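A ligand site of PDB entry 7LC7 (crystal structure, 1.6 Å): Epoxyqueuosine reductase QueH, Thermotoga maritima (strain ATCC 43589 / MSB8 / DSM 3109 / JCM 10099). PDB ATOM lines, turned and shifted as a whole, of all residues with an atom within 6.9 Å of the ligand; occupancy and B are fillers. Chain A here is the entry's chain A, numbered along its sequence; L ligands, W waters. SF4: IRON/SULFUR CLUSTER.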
ATOM      1  N   ASN A  32      -1.158  -2.037   2.236  1.00  0.00           N
ATOM      2  CA  ASN A  32      -0.848  -1.461   3.541  1.00  0.00           C
ATOM      3  C   ASN A  32      -0.397  -0.010   3.440  1.00  0.00           C
ATOM      4  O   ASN A  32      -0.358   0.685   4.459  1.00  0.00           O
ATOM      5  CB  ASN A  32       0.251  -2.252   4.232  1.00  0.00           C
ATOM      6  CG  ASN A  32       1.477  -2.429   3.371  1.00  0.00           C
ATOM      7  OD1 ASN A  32       1.374  -2.833   2.203  1.00  0.00           O
ATOM      8  ND2 ASN A  32       2.645  -2.141   3.920  1.00  0.00           N
ATOM      9  N   ILE A  33      -0.031   0.463   2.245  1.00  0.00           N
ATOM     10  CA  ILE A  33       0.443   1.826   2.092  1.00  0.00           C
ATOM     11  C   ILE A  33      -0.752   2.747   1.919  1.00  0.00           C
ATOM     12  O   ILE A  33      -1.520   2.623   0.954  1.00  0.00           O
ATOM     13  CB  ILE A  33       1.400   1.968   0.917  1.00  0.00           C
ATOM     14  CG1 ILE A  33       2.657   1.135   1.122  1.00  0.00           C
ATOM     15  CG2 ILE A  33       1.766   3.450   0.726  1.00  0.00           C
ATOM     16  CD1 ILE A  33       3.536   1.063  -0.104  1.00  0.00           C
ATOM     17  N   TRP A  70      -6.766  -5.898   3.827  1.00  0.00           N
ATOM     18  CA  TRP A  70      -5.574  -5.776   4.647  1.00  0.00           C
ATOM     19  C   TRP A  70      -5.930  -5.309   6.053  1.00  0.00           C
ATOM     20  O   TRP A  70      -5.415  -5.853   7.045  1.00  0.00           O
ATOM     21  CB  TRP A  70      -4.571  -4.806   4.005  1.00  0.00           C
ATOM     22  CG  TRP A  70      -3.435  -4.447   4.922  1.00  0.00           C
ATOM     23  CD1 TRP A  70      -2.285  -5.161   5.111  1.00  0.00           C
ATOM     24  CD2 TRP A  70      -3.345  -3.306   5.773  1.00  0.00           C
ATOM     25  NE1 TRP A  70      -1.488  -4.532   6.036  1.00  0.00           N
ATOM     26  CE2 TRP A  70      -2.114  -3.393   6.457  1.00  0.00           C
ATOM     27  CE3 TRP A  70      -4.189  -2.208   6.037  1.00  0.00           C
ATOM     28  CZ2 TRP A  70      -1.700  -2.426   7.377  1.00  0.00           C
ATOM     29  CZ3 TRP A  70      -3.775  -1.267   6.950  1.00  0.00           C
ATOM     30  CH2 TRP A  70      -2.538  -1.377   7.607  1.00  0.00           C
ATOM     31  N   VAL A  74      -5.062  -6.948  10.114  1.00  0.00           N
ATOM     32  CA  VAL A  74      -4.238  -6.310  11.135  1.00  0.00           C
ATOM     33  C   VAL A  74      -5.057  -5.629  12.220  1.00  0.00           C
ATOM     34  O   VAL A  74      -4.486  -5.281  13.261  1.00  0.00           O
ATOM     35  CB  VAL A  74      -3.267  -5.287  10.511  1.00  0.00           C
ATOM     36  CG1 VAL A  74      -2.432  -5.939   9.428  1.00  0.00           C
ATOM     37  CG2 VAL A  74      -4.025  -4.097   9.943  1.00  0.00           C
ATOM     38  N   GLY A  81       2.652  -1.523  18.572  1.00  0.00           N
ATOM     39  CA  GLY A  81       3.574  -0.754  17.775  1.00  0.00           C
ATOM     40  C   GLY A  81       4.169  -1.554  16.627  1.00  0.00           C
ATOM     41  O   GLY A  81       3.826  -2.708  16.393  1.00  0.00           O
ATOM     42  N   GLU A  82       5.070  -0.891  15.891  1.00  0.00           N
ATOM     43  CA  GLU A  82       5.815  -1.575  14.839  1.00  0.00           C
ATOM     44  C   GLU A  82       6.760  -2.597  15.453  1.00  0.00           C
ATOM     45  O   GLU A  82       7.411  -2.339  16.478  1.00  0.00           O
ATOM     46  CB  GLU A  82       6.602  -0.572  13.987  1.00  0.00           C
ATOM     47  CG  GLU A  82       7.726  -1.228  13.174  1.00  0.00           C
ATOM     48  CD  GLU A  82       8.089  -0.475  11.899  1.00  0.00           C
ATOM     49  OE1 GLU A  82       8.544  -1.123  10.930  1.00  0.00           O
ATOM     50  OE2 GLU A  82       7.926   0.765  11.872  1.00  0.00           O
ATOM     51  N   GLY A  83       6.839  -3.762  14.823  1.00  0.00           N
ATOM     52  CA  GLY A  83       7.606  -4.886  15.316  1.00  0.00           C
ATOM     53  C   GLY A  83       6.781  -5.923  16.051  1.00  0.00           C
ATOM     54  O   GLY A  83       7.308  -6.997  16.376  1.00  0.00           O
ATOM     55  N   SER A  84       5.502  -5.655  16.278  1.00  0.00           N
ATOM     56  CA  SER A  84       4.638  -6.494  17.092  1.00  0.00           C
ATOM     57  C   SER A  84       3.860  -7.482  16.218  1.00  0.00           C
ATOM     58  O   SER A  84       4.173  -7.690  15.037  1.00  0.00           O
ATOM     59  CB  SER A  84       3.699  -5.615  17.912  1.00  0.00           C
ATOM     60  OG  SER A  84       2.790  -4.928  17.060  1.00  0.00           O
ATOM     61  N   ARG A  86       1.093  -6.993  14.990  1.00  0.00           N
ATOM     62  CA  ARG A  86       0.473  -6.281  13.867  1.00  0.00           C
ATOM     63  C   ARG A  86       1.319  -6.427  12.612  1.00  0.00           C
ATOM     64  O   ARG A  86       0.788  -6.680  11.523  1.00  0.00           O
ATOM     65  CB  ARG A  86       0.287  -4.809  14.235  1.00  0.00           C
ATOM     66  CG  ARG A  86      -0.311  -3.937  13.144  1.00  0.00           C
ATOM     67  CD  ARG A  86      -0.173  -2.456  13.504  1.00  0.00           C
ATOM     68  NE  ARG A  86       1.141  -1.916  13.155  1.00  0.00           N
ATOM     69  CZ  ARG A  86       1.690  -0.836  13.714  1.00  0.00           C
ATOM     70  NH1 ARG A  86       1.042  -0.180  14.666  1.00  0.00           N
ATOM     71  NH2 ARG A  86       2.890  -0.407  13.334  1.00  0.00           N
ATOM     72  N   CYS A  87       2.631  -6.281  12.739  1.00  0.00           N
ATOM     73  CA  CYS A  87       3.493  -6.414  11.567  1.00  0.00           C
ATOM     74  C   CYS A  87       3.600  -7.850  11.092  1.00  0.00           C
ATOM     75  O   CYS A  87       3.741  -8.085   9.889  1.00  0.00           O
ATOM     76  CB  CYS A  87       4.870  -5.831  11.872  1.00  0.00           C
ATOM     77  SG  CYS A  87       4.730  -4.139  12.477  1.00  0.00           S
ATOM     78  N   GLU A  88       3.572  -8.811  12.010  1.00  0.00           N
ATOM     79  CA  GLU A  88       3.522 -10.204  11.580  1.00  0.00           C
ATOM     80  C   GLU A  88       2.310 -10.456  10.696  1.00  0.00           C
ATOM     81  O   GLU A  88       2.423 -11.116   9.663  1.00  0.00           O
ATOM     82  CB  GLU A  88       3.509 -11.131  12.792  1.00  0.00           C
ATOM     83  CG  GLU A  88       3.413 -12.601  12.446  1.00  0.00           C
ATOM     84  CD  GLU A  88       3.737 -13.491  13.630  1.00  0.00           C
ATOM     85  OE1 GLU A  88       3.750 -12.978  14.773  1.00  0.00           O
ATOM     86  OE2 GLU A  88       3.994 -14.703  13.411  1.00  0.00           O
ATOM     87  N   ARG A  89       1.152  -9.921  11.077  1.00  0.00           N
ATOM     88  CA  ARG A  89      -0.045 -10.118  10.287  1.00  0.00           C
ATOM     89  C   ARG A  89       0.034  -9.403   8.946  1.00  0.00           C
ATOM     90  O   ARG A  89      -0.411  -9.923   7.922  1.00  0.00           O
ATOM     91  CB  ARG A  89      -1.264  -9.625  11.070  1.00  0.00           C
ATOM     92  CG  ARG A  89      -2.025 -10.711  11.829  1.00  0.00           C
ATOM     93  CD  ARG A  89      -2.308 -11.915  10.950  1.00  0.00           C
ATOM     94  NE  ARG A  89      -2.645 -11.564   9.563  1.00  0.00           N
ATOM     95  CZ  ARG A  89      -2.338 -12.326   8.521  1.00  0.00           C
ATOM     96  NH1 ARG A  89      -1.714 -13.484   8.707  1.00  0.00           N
ATOM     97  NH2 ARG A  89      -2.663 -11.954   7.293  1.00  0.00           N
ATOM     98  N   CYS A  90       0.605  -8.202   8.955  1.00  0.00           N
ATOM     99  CA  CYS A  90       0.717  -7.416   7.729  1.00  0.00           C
ATOM    100  C   CYS A  90       1.619  -8.102   6.718  1.00  0.00           C
ATOM    101  O   CYS A  90       1.261  -8.280   5.537  1.00  0.00           O
ATOM    102  CB  CYS A  90       1.241  -6.033   8.100  1.00  0.00           C
ATOM    103  SG  CYS A  90       1.646  -5.011   6.689  1.00  0.00           S
ATOM    104  N   ILE A  91       2.799  -8.526   7.161  1.00  0.00           N
ATOM    105  CA  ILE A  91       3.755  -9.133   6.242  1.00  0.00           C
ATOM    106  C   ILE A  91       3.241 -10.477   5.755  1.00  0.00           C
ATOM    107  O   ILE A  91       3.445 -10.861   4.590  1.00  0.00           O
ATOM    108  CB  ILE A  91       5.134  -9.231   6.919  1.00  0.00           C
ATOM    109  CG1 ILE A  91       5.684  -7.817   7.135  1.00  0.00           C
ATOM    110  CG2 ILE A  91       6.077 -10.075   6.057  1.00  0.00           C
ATOM    111  CD1 ILE A  91       6.919  -7.739   8.039  1.00  0.00           C
ATOM    112  N   LEU A  94       0.829  -9.779   2.919  1.00  0.00           N
ATOM    113  CA  LEU A  94       1.521  -9.459   1.671  1.00  0.00           C
ATOM    114  C   LEU A  94       2.158 -10.695   1.074  1.00  0.00           C
ATOM    115  O   LEU A  94       2.113 -10.902  -0.138  1.00  0.00           O
ATOM    116  CB  LEU A  94       2.583  -8.400   1.932  1.00  0.00           C
ATOM    117  CG  LEU A  94       2.052  -7.060   2.480  1.00  0.00           C
ATOM    118  CD1 LEU A  94       3.185  -6.114   2.781  1.00  0.00           C
ATOM    119  CD2 LEU A  94       1.062  -6.435   1.501  1.00  0.00           C
ATOM    120  N   LEU A 114      11.449  -6.978   1.404  1.00  0.00           N
ATOM    121  CA  LEU A 114      11.465  -6.651   2.837  1.00  0.00           C
ATOM    122  C   LEU A 114      12.681  -7.257   3.506  1.00  0.00           C
ATOM    123  O   LEU A 114      13.147  -6.745   4.533  1.00  0.00           O
ATOM    124  CB  LEU A 114      10.180  -7.142   3.509  1.00  0.00           C
ATOM    125  CG  LEU A 114       8.860  -6.437   3.154  1.00  0.00           C
ATOM    126  CD1 LEU A 114       7.691  -7.285   3.614  1.00  0.00           C
ATOM    127  CD2 LEU A 114       8.823  -5.063   3.802  1.00  0.00           C
ATOM    128  N   LYS A 120      13.366  -4.172   9.376  1.00  0.00           N
ATOM    129  CA  LYS A 120      12.509  -5.324   9.584  1.00  0.00           C
ATOM    130  C   LYS A 120      13.228  -6.431  10.349  1.00  0.00           C
ATOM    131  O   LYS A 120      14.449  -6.472  10.483  1.00  0.00           O
ATOM    132  CB  LYS A 120      11.985  -5.841   8.238  1.00  0.00           C
ATOM    133  CG  LYS A 120      11.201  -4.809   7.422  1.00  0.00           C
ATOM    134  CD  LYS A 120       9.791  -4.621   7.947  1.00  0.00           C
ATOM    135  CE  LYS A 120       9.400  -3.145   8.001  1.00  0.00           C
ATOM    136  NZ  LYS A 120       9.970  -2.347   6.871  1.00  0.00           N
ATOM    137  N   MET A 124      11.516 -13.002  11.934  1.00  0.00           N
ATOM    138  CA  MET A 124      10.073 -12.966  11.727  1.00  0.00           C
ATOM    139  C   MET A 124       9.727 -13.180  10.259  1.00  0.00           C
ATOM    140  O   MET A 124       8.829 -13.966   9.928  1.00  0.00           O
ATOM    141  CB  MET A 124       9.499 -11.624  12.211  1.00  0.00           C
ATOM    142  CG  MET A 124       8.073 -11.383  11.723  1.00  0.00           C
ATOM    143  SD  MET A 124       7.377  -9.751  12.086  1.00  0.00           S
ATOM    144  CE  MET A 124       8.445  -8.667  11.151  1.00  0.00           C
ATOM    145  N   TYR A 168       8.459   6.505   6.638  1.00  0.00           N
ATOM    146  CA  TYR A 168       7.586   5.712   7.496  1.00  0.00           C
ATOM    147  C   TYR A 168       7.238   4.426   6.769  1.00  0.00           C
ATOM    148  O   TYR A 168       7.244   4.382   5.532  1.00  0.00           O
ATOM    149  CB  TYR A 168       6.324   6.481   7.927  1.00  0.00           C
ATOM    150  CG  TYR A 168       5.270   6.752   6.872  1.00  0.00           C
ATOM    151  CD1 TYR A 168       5.489   7.679   5.856  1.00  0.00           C
ATOM    152  CD2 TYR A 168       4.033   6.129   6.927  1.00  0.00           C
ATOM    153  CE1 TYR A 168       4.510   7.937   4.903  1.00  0.00           C
ATOM    154  CE2 TYR A 168       3.052   6.384   5.983  1.00  0.00           C
ATOM    155  CZ  TYR A 168       3.289   7.301   4.980  1.00  0.00           C
ATOM    156  OH  TYR A 168       2.296   7.544   4.051  1.00  0.00           O
ATOM    157  N   CYS A 169       6.942   3.388   7.549  1.00  0.00           N
ATOM    158  CA  CYS A 169       6.865   2.043   6.976  1.00  0.00           C
ATOM    159  C   CYS A 169       5.829   1.969   5.868  1.00  0.00           C
ATOM    160  O   CYS A 169       6.095   1.447   4.777  1.00  0.00           O
ATOM    161  CB  CYS A 169       6.572   1.027   8.065  1.00  0.00           C
ATOM    162  SG  CYS A 169       6.909  -0.614   7.474  1.00  0.00           S
ATOM    163  N   GLY A 170       4.624   2.490   6.114  1.00  0.00           N
ATOM    164  CA  GLY A 170       3.655   2.635   5.044  1.00  0.00           C
ATOM    165  C   GLY A 170       2.226   2.778   5.518  1.00  0.00           C
ATOM    166  O   GLY A 170       1.427   3.496   4.898  1.00  0.00           O
ATOM    167  N   CYS A 171       1.864   2.101   6.601  1.00  0.00           N
ATOM    168  CA  CYS A 171       0.476   2.118   7.005  1.00  0.00           C
ATOM    169  C   CYS A 171       0.167   3.345   7.860  1.00  0.00           C
ATOM    170  O   CYS A 171       1.068   4.060   8.311  1.00  0.00           O
ATOM    171  CB  CYS A 171       0.126   0.859   7.782  1.00  0.00           C
ATOM    172  SG  CYS A 171       0.869   0.856   9.423  1.00  0.00           S
ATOM    173  N   VAL A 172      -1.129   3.568   8.091  1.00  0.00           N
ATOM    174  CA  VAL A 172      -1.552   4.729   8.864  1.00  0.00           C
ATOM    175  C   VAL A 172      -0.990   4.652  10.284  1.00  0.00           C
ATOM    176  O   VAL A 172      -0.612   5.678  10.867  1.00  0.00           O
ATOM    177  CB  VAL A 172      -3.093   4.831   8.854  1.00  0.00           C
ATOM    178  CG1 VAL A 172      -3.720   3.559   9.423  1.00  0.00           C
ATOM    179  CG2 VAL A 172      -3.537   6.054   9.638  1.00  0.00           C
ATOM    180  N   PHE A 173      -0.911   3.442  10.846  1.00  0.00           N
ATOM    181  CA  PHE A 173      -0.355   3.291  12.190  1.00  0.00           C
ATOM    182  C   PHE A 173       1.081   3.770  12.243  1.00  0.00           C
ATOM    183  O   PHE A 173       1.468   4.502  13.163  1.00  0.00           O
ATOM    184  CB  PHE A 173      -0.448   1.832  12.633  1.00  0.00           C
ATOM    185  CG  PHE A 173      -1.775   1.198  12.381  1.00  0.00           C
ATOM    186  CD1 PHE A 173      -2.925   1.723  12.955  1.00  0.00           C
ATOM    187  CD2 PHE A 173      -1.880   0.083  11.566  1.00  0.00           C
ATOM    188  CE1 PHE A 173      -4.156   1.141  12.711  1.00  0.00           C
ATOM    189  CE2 PHE A 173      -3.114  -0.502  11.331  1.00  0.00           C
ATOM    190  CZ  PHE A 173      -4.247   0.025  11.899  1.00  0.00           C
ATOM    191  N   SER A 174       1.891   3.386  11.253  1.00  0.00           N
ATOM    192  CA  SER A 174       3.299   3.784  11.254  1.00  0.00           C
ATOM    193  C   SER A 174       3.445   5.289  11.042  1.00  0.00           C
ATOM    194  O   SER A 174       4.410   5.884  11.530  1.00  0.00           O
ATOM    195  CB  SER A 174       4.053   3.011  10.178  1.00  0.00           C
ATOM    196  OG  SER A 174       3.571   3.317   8.889  1.00  0.00           O
ATOM    197  N   GLU A 177       2.864   6.767  14.532  1.00  0.00           N
ATOM    198  CA  GLU A 177       4.013   6.483  15.384  1.00  0.00           C
ATOM    199  C   GLU A 177       5.213   7.331  14.975  1.00  0.00           C
ATOM    200  O   GLU A 177       6.058   7.645  15.822  1.00  0.00           O
ATOM    201  CB  GLU A 177       4.332   4.991  15.326  1.00  0.00           C
ATOM    202  CG  GLU A 177       3.184   4.121  15.840  1.00  0.00           C
ATOM    203  CD  GLU A 177       3.116   2.757  15.177  1.00  0.00           C
ATOM    204  OE1 GLU A 177       4.127   2.307  14.587  1.00  0.00           O
ATOM    205  OE2 GLU A 177       2.046   2.114  15.260  1.00  0.00           O
HETATM  206 FE1  SF4 L   1       4.820  -1.685   8.287  1.00  0.00          FE
HETATM  207 FE2  SF4 L   1       3.886  -3.006  10.427  1.00  0.00          FE
HETATM  208 FE3  SF4 L   1       2.771  -3.346   8.026  1.00  0.00          FE
HETATM  209 FE4  SF4 L   1       2.414  -1.043   9.288  1.00  0.00          FE
HETATM  210  S1  SF4 L   1       1.665  -3.053   9.986  1.00  0.00           S
HETATM  211  S2  SF4 L   1       2.952  -1.296   7.068  1.00  0.00           S
HETATM  212  S3  SF4 L   1       4.403  -0.792  10.360  1.00  0.00           S
HETATM  213  S4  SF4 L   1       4.893  -3.944   8.607  1.00  0.00           S
HETATM  214  O   HOH W   1       5.470  -4.339   5.291  1.00  0.00           O
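The side-chain sulfur (SG) of Cys 90 is bound to an iron atom (FE3) of the ligand. The backbone NH (N) of Cys 171 sits close to a sulfur (S2) of the ligand (3.6 Å). An iron atom (FE4) of the ligand is bound by the side-chain sulfur (SG) of Cys 171, 2.5 Å away. The side-chain sulfur of Cys 169 binds an iron atom (FE1) of the ligand, 2.5 Å away. FE2 of the ligand is bound by SG of Cys 87, at 2.5 Å. ND2 of Asn 32 sits close to S2 of the ligand. A sulfur (S3) of the ligand sits close to the guanidinium group of Arg 86 (3.4 Å).
The indole nitrogen (NE1) of Trp 70 lies close to the side-chain sulfur (SG) of Cys 90, 3.2 Å away. The backbone NH (N) of Cys 171 lies close to the backbone carbonyl oxygen (O) of Asn 32, at 3.4 Å. The side-chain hydroxyl (OG) of Ser 174 lies within hydrogen-bond range of the backbone carbonyl oxygen (O) of Cys 171 (2.7 Å). The side-chain sulfur of Cys 171 lies close to the backbone NH of Phe 173, at 3.4 Å. The side-chain sulfur (SG) of Cys 169 sits close to the side-chain amino group (NZ) of Lys 120 (3.6 Å). The side-chain sulfur of Cys 87 sits close to the backbone NH of Gly 83. The guanidinium group of Arg 86 is in salt-bridge range of the side-chain carboxylate of Glu 177, 2.6 Å away. The side-chain hydroxyl (OG) of Ser 174 is in hydrogen-bond range of the backbone NH (N) of Gly 170.
Ser 174 touches the ligand. Of the 26 residues printed, 7 come within 4 Å of the ligand.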
